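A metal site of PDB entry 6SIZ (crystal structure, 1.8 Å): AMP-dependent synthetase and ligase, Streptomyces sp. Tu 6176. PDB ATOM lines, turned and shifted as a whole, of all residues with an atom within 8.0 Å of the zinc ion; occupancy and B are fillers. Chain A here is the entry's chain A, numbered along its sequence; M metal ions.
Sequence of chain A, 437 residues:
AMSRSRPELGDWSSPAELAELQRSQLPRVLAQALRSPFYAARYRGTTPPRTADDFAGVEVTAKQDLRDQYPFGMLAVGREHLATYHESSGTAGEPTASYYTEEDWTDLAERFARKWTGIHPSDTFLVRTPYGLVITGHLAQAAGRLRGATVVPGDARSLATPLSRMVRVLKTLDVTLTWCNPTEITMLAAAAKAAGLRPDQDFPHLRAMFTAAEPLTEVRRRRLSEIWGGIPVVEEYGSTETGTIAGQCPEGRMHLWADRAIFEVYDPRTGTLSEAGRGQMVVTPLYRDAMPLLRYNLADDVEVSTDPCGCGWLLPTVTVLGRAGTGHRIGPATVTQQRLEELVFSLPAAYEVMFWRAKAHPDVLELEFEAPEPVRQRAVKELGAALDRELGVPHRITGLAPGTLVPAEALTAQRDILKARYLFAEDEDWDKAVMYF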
ATOM      1  N   GLY A 247     -14.880   5.214   8.166  1.00  0.00           N
ATOM      2  CA  GLY A 247     -13.519   4.773   7.802  1.00  0.00           C
ATOM      3  C   GLY A 247     -13.367   3.279   7.844  1.00  0.00           C
ATOM      4  O   GLY A 247     -14.009   2.633   8.720  1.00  0.00           O
ATOM      5  N   GLN A 248     -12.501   2.742   6.994  1.00  0.00           N
ATOM      6  CA  GLN A 248     -12.189   1.294   6.871  1.00  0.00           C
ATOM      7  C   GLN A 248     -11.535   0.741   8.156  1.00  0.00           C
ATOM      8  O   GLN A 248     -10.675   1.437   8.728  1.00  0.00           O
ATOM      9  CB  GLN A 248     -11.263   1.094   5.675  1.00  0.00           C
ATOM     10  CG  GLN A 248     -11.074  -0.368   5.292  1.00  0.00           C
ATOM     11  CD  GLN A 248     -10.069  -0.536   4.190  1.00  0.00           C
ATOM     12  OE1 GLN A 248      -8.886  -0.763   4.414  1.00  0.00           O
ATOM     13  NE2 GLN A 248     -10.553  -0.393   2.966  1.00  0.00           N
ATOM     14  N   CYS A 249     -11.906  -0.473   8.586  1.00  0.00           N
ATOM     15  CA  CYS A 249     -11.161  -1.258   9.609  1.00  0.00           C
ATOM     16  C   CYS A 249     -10.178  -2.197   8.899  1.00  0.00           C
ATOM     17  O   CYS A 249     -10.263  -2.381   7.693  1.00  0.00           O
ATOM     18  CB  CYS A 249     -12.116  -2.062  10.491  1.00  0.00           C
ATOM     19  SG  CYS A 249     -12.980  -3.357   9.561  1.00  0.00           S
ATOM     20  N   PRO A 250      -9.256  -2.889   9.622  1.00  0.00           N
ATOM     21  CA  PRO A 250      -8.347  -3.843   8.978  1.00  0.00           C
ATOM     22  C   PRO A 250      -9.051  -5.032   8.281  1.00  0.00           C
ATOM     23  O   PRO A 250      -8.416  -5.656   7.441  1.00  0.00           O
ATOM     24  CB  PRO A 250      -7.454  -4.347  10.128  1.00  0.00           C
ATOM     25  CG  PRO A 250      -7.620  -3.329  11.237  1.00  0.00           C
ATOM     26  CD  PRO A 250      -9.015  -2.758  11.066  1.00  0.00           C
ATOM     27  N   GLU A 251     -10.332  -5.277   8.582  1.00  0.00           N
ATOM     28  CA  GLU A 251     -11.145  -6.343   7.941  1.00  0.00           C
ATOM     29  C   GLU A 251     -11.742  -5.859   6.613  1.00  0.00           C
ATOM     30  O   GLU A 251     -12.298  -6.688   5.878  1.00  0.00           O
ATOM     31  CB  GLU A 251     -12.251  -6.802   8.888  1.00  0.00           C
ATOM     32  CG  GLU A 251     -11.708  -7.350  10.193  1.00  0.00           C
ATOM     33  CD  GLU A 251     -10.706  -8.480   9.981  1.00  0.00           C
ATOM     34  OE1 GLU A 251      -9.539  -8.320  10.392  1.00  0.00           O
ATOM     35  OE2 GLU A 251     -11.094  -9.504   9.390  1.00  0.00           O
ATOM     36  N   GLY A 252     -11.652  -4.555   6.313  1.00  0.00           N
ATOM     37  CA  GLY A 252     -11.987  -4.004   4.978  1.00  0.00           C
ATOM     38  C   GLY A 252     -13.393  -3.450   4.895  1.00  0.00           C
ATOM     39  O   GLY A 252     -13.799  -3.079   3.783  1.00  0.00           O
ATOM     40  N   ARG A 253     -14.113  -3.344   6.019  1.00  0.00           N
ATOM     41  CA  ARG A 253     -15.447  -2.697   6.095  1.00  0.00           C
ATOM     42  C   ARG A 253     -15.287  -1.255   6.613  1.00  0.00           C
ATOM     43  O   ARG A 253     -14.413  -1.008   7.468  1.00  0.00           O
ATOM     44  CB  ARG A 253     -16.384  -3.477   7.033  1.00  0.00           C
ATOM     45  CG  ARG A 253     -16.723  -4.882   6.569  1.00  0.00           C
ATOM     46  CD  ARG A 253     -17.824  -5.484   7.434  1.00  0.00           C
ATOM     47  NE  ARG A 253     -17.864  -6.939   7.445  1.00  0.00           N
ATOM     48  CZ  ARG A 253     -18.855  -7.664   7.966  1.00  0.00           C
ATOM     49  NH1 ARG A 253     -18.791  -8.978   7.930  1.00  0.00           N
ATOM     50  NH2 ARG A 253     -19.908  -7.082   8.508  1.00  0.00           N
ATOM     51  N   MET A 254     -16.116  -0.333   6.120  1.00  0.00           N
ATOM     52  CA  MET A 254     -16.191   1.050   6.626  1.00  0.00           C
ATOM     53  C   MET A 254     -17.128   1.077   7.847  1.00  0.00           C
ATOM     54  O   MET A 254     -18.257   0.599   7.719  1.00  0.00           O
ATOM     55  CB  MET A 254     -16.686   2.029   5.565  1.00  0.00           C
ATOM     56  CG  MET A 254     -15.656   2.275   4.476  1.00  0.00           C
ATOM     57  SD  MET A 254     -16.016   3.740   3.446  1.00  0.00           S
ATOM     58  CE  MET A 254     -17.525   3.212   2.639  1.00  0.00           C
ATOM     59  N   HIS A 255     -16.653   1.619   8.962  1.00  0.00           N
ATOM     60  CA  HIS A 255     -17.435   1.831  10.209  1.00  0.00           C
ATOM     61  C   HIS A 255     -17.811   3.310  10.321  1.00  0.00           C
ATOM     62  O   HIS A 255     -16.954   4.175  10.049  1.00  0.00           O
ATOM     63  CB  HIS A 255     -16.603   1.349  11.387  1.00  0.00           C
ATOM     64  CG  HIS A 255     -16.475  -0.138  11.473  1.00  0.00           C
ATOM     65  ND1 HIS A 255     -17.219  -0.874  12.356  1.00  0.00           N
ATOM     66  CD2 HIS A 255     -15.688  -1.015  10.819  1.00  0.00           C
ATOM     67  CE1 HIS A 255     -16.916  -2.141  12.239  1.00  0.00           C
ATOM     68  NE2 HIS A 255     -15.987  -2.273  11.309  1.00  0.00           N
ATOM     69  N   ASP A 307     -24.300  -5.473  12.742  1.00  0.00           N
ATOM     70  CA  ASP A 307     -23.659  -6.813  12.913  1.00  0.00           C
ATOM     71  C   ASP A 307     -22.209  -6.633  13.362  1.00  0.00           C
ATOM     72  O   ASP A 307     -21.468  -5.856  12.770  1.00  0.00           O
ATOM     73  CB  ASP A 307     -23.679  -7.642  11.620  1.00  0.00           C
ATOM     74  CG  ASP A 307     -25.030  -8.232  11.270  1.00  0.00           C
ATOM     75  OD1 ASP A 307     -25.899  -8.288  12.162  1.00  0.00           O
ATOM     76  OD2 ASP A 307     -25.199  -8.632  10.091  1.00  0.00           O
ATOM     77  N   PRO A 308     -21.738  -7.377  14.396  1.00  0.00           N
ATOM     78  CA  PRO A 308     -20.378  -7.193  14.890  1.00  0.00           C
ATOM     79  C   PRO A 308     -19.364  -7.554  13.789  1.00  0.00           C
ATOM     80  O   PRO A 308     -19.702  -8.357  12.908  1.00  0.00           O
ATOM     81  CB  PRO A 308     -20.288  -8.135  16.097  1.00  0.00           C
ATOM     82  CG  PRO A 308     -21.343  -9.195  15.822  1.00  0.00           C
ATOM     83  CD  PRO A 308     -22.442  -8.472  15.083  1.00  0.00           C
ATOM     84  N   CYS A 309     -18.189  -6.933  13.835  1.00  0.00           N
ATOM     85  CA  CYS A 309     -17.092  -7.111  12.853  1.00  0.00           C
ATOM     86  C   CYS A 309     -15.887  -7.729  13.565  1.00  0.00           C
ATOM     87  O   CYS A 309     -15.706  -7.456  14.776  1.00  0.00           O
ATOM     88  CB  CYS A 309     -16.731  -5.777  12.188  1.00  0.00           C
ATOM     89  SG  CYS A 309     -15.644  -5.959  10.763  1.00  0.00           S
ATOM     90  N   GLY A 310     -15.097  -8.536  12.833  1.00  0.00           N
ATOM     91  CA  GLY A 310     -13.873  -9.188  13.339  1.00  0.00           C
ATOM     92  C   GLY A 310     -12.832  -8.199  13.852  1.00  0.00           C
ATOM     93  O   GLY A 310     -11.952  -8.630  14.597  1.00  0.00           O
ATOM     94  N   CYS A 311     -12.925  -6.920  13.465  1.00  0.00           N
ATOM     95  CA  CYS A 311     -12.001  -5.826  13.887  1.00  0.00           C
ATOM     96  C   CYS A 311     -12.218  -5.461  15.369  1.00  0.00           C
ATOM     97  O   CYS A 311     -11.271  -4.937  15.988  1.00  0.00           O
ATOM     98  CB  CYS A 311     -12.180  -4.585  13.019  1.00  0.00           C
ATOM     99  SG  CYS A 311     -13.680  -3.638  13.384  1.00  0.00           S
ATOM    100  N   GLY A 312     -13.425  -5.692  15.894  1.00  0.00           N
ATOM    101  CA  GLY A 312     -13.769  -5.471  17.320  1.00  0.00           C
ATOM    102  C   GLY A 312     -14.115  -4.022  17.623  1.00  0.00           C
ATOM    103  O   GLY A 312     -14.424  -3.742  18.789  1.00  0.00           O
ATOM    104  N   TRP A 313     -14.084  -3.105  16.664  1.00  0.00           N
ATOM    105  CA  TRP A 313     -14.615  -1.726  16.844  1.00  0.00           C
ATOM    106  C   TRP A 313     -16.118  -1.815  17.098  1.00  0.00           C
ATOM    107  O   TRP A 313     -16.808  -2.477  16.310  1.00  0.00           O
ATOM    108  CB  TRP A 313     -14.373  -0.837  15.612  1.00  0.00           C
ATOM    109  CG  TRP A 313     -12.951  -0.648  15.197  1.00  0.00           C
ATOM    110  CD1 TRP A 313     -11.836  -1.079  15.847  1.00  0.00           C
ATOM    111  CD2 TRP A 313     -12.496   0.079  14.048  1.00  0.00           C
ATOM    112  NE1 TRP A 313     -10.713  -0.693  15.159  1.00  0.00           N
ATOM    113  CE2 TRP A 313     -11.087   0.018  14.056  1.00  0.00           C
ATOM    114  CE3 TRP A 313     -13.146   0.755  13.011  1.00  0.00           C
ATOM    115  CZ2 TRP A 313     -10.316   0.612  13.062  1.00  0.00           C
ATOM    116  CZ3 TRP A 313     -12.378   1.357  12.032  1.00  0.00           C
ATOM    117  CH2 TRP A 313     -10.983   1.284  12.064  1.00  0.00           C
ATOM    118  N   LEU A 314     -16.616  -1.124  18.132  1.00  0.00           N
ATOM    119  CA  LEU A 314     -18.051  -1.156  18.524  1.00  0.00           C
ATOM    120  C   LEU A 314     -18.784  -0.062  17.763  1.00  0.00           C
ATOM    121  O   LEU A 314     -19.283   0.901  18.385  1.00  0.00           O
ATOM    122  CB  LEU A 314     -18.160  -1.022  20.049  1.00  0.00           C
ATOM    123  CG  LEU A 314     -17.509  -2.170  20.822  1.00  0.00           C
ATOM    124  CD1 LEU A 314     -17.618  -1.965  22.315  1.00  0.00           C
ATOM    125  CD2 LEU A 314     -18.098  -3.520  20.420  1.00  0.00           C
ATOM    126  N   LEU A 315     -18.815  -0.201  16.430  1.00  0.00           N
ATOM    127  CA  LEU A 315     -19.445   0.781  15.519  1.00  0.00           C
ATOM    128  C   LEU A 315     -20.131   0.037  14.381  1.00  0.00           C
ATOM    129  O   LEU A 315     -19.581  -0.920  13.853  1.00  0.00           O
ATOM    130  CB  LEU A 315     -18.361   1.708  14.974  1.00  0.00           C
ATOM    131  CG  LEU A 315     -17.756   2.687  15.972  1.00  0.00           C
ATOM    132  CD1 LEU A 315     -16.552   3.371  15.373  1.00  0.00           C
ATOM    133  CD2 LEU A 315     -18.787   3.708  16.426  1.00  0.00           C
ATOM    134  N   PRO A 316     -21.340   0.453  13.960  1.00  0.00           N
ATOM    135  CA  PRO A 316     -21.981  -0.125  12.782  1.00  0.00           C
ATOM    136  C   PRO A 316     -21.150   0.112  11.506  1.00  0.00           C
ATOM    137  O   PRO A 316     -20.399   1.083  11.462  1.00  0.00           O
ATOM    138  CB  PRO A 316     -23.331   0.587  12.684  1.00  0.00           C
ATOM    139  CG  PRO A 316     -23.131   1.873  13.471  1.00  0.00           C
ATOM    140  CD  PRO A 316     -22.147   1.527  14.562  1.00  0.00           C
ATOM    141  N   THR A 317     -21.270  -0.794  10.535  1.00  0.00           N
ATOM    142  CA  THR A 317     -20.576  -0.745   9.226  1.00  0.00           C
ATOM    143  C   THR A 317     -21.517  -0.088   8.210  1.00  0.00           C
ATOM    144  O   THR A 317     -22.721  -0.048   8.465  1.00  0.00           O
ATOM    145  CB  THR A 317     -20.127  -2.148   8.780  1.00  0.00           C
ATOM    146  OG1 THR A 317     -21.314  -2.926   8.643  1.00  0.00           O
ATOM    147  CG2 THR A 317     -19.174  -2.807   9.747  1.00  0.00           C
HETATM  148 ZN    ZN M   1     -14.486  -3.749  11.128  1.00  0.00          ZN
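The zinc ion is bound by a ring nitrogen (NE2) of His 255 (2.1 Å), the side-chain sulfur of Cys 249 (2.2 Å), the side-chain sulfur of Cys 311 (2.4 Å) and the side-chain sulfur of Cys 309 (2.5 Å).
Of the 20 residues printed, 4 come within 4 Å of the zinc ion.
The backbone NH (N) of His 255 is in hydrogen-bond range of the backbone carbonyl oxygen (O) of Gly 247 (2.8 Å). SG of Cys 311 lies close to N of Trp 313, 3.3 Å away. The side-chain sulfur of Cys 249 lies close to the backbone carbonyl oxygen of Arg 253, at 3.5 Å. N of Glu 251 lies close to SG of Cys 249, 3.4 Å away. The backbone carbonyl oxygen (O) of Leu 315 lies within hydrogen-bond range of a ring nitrogen (ND1) of His 255, at 2.8 Å. The side-chain sulfur (SG) of Cys 249 sits close to the backbone NH (N) of Gly 252 (3.7 Å).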
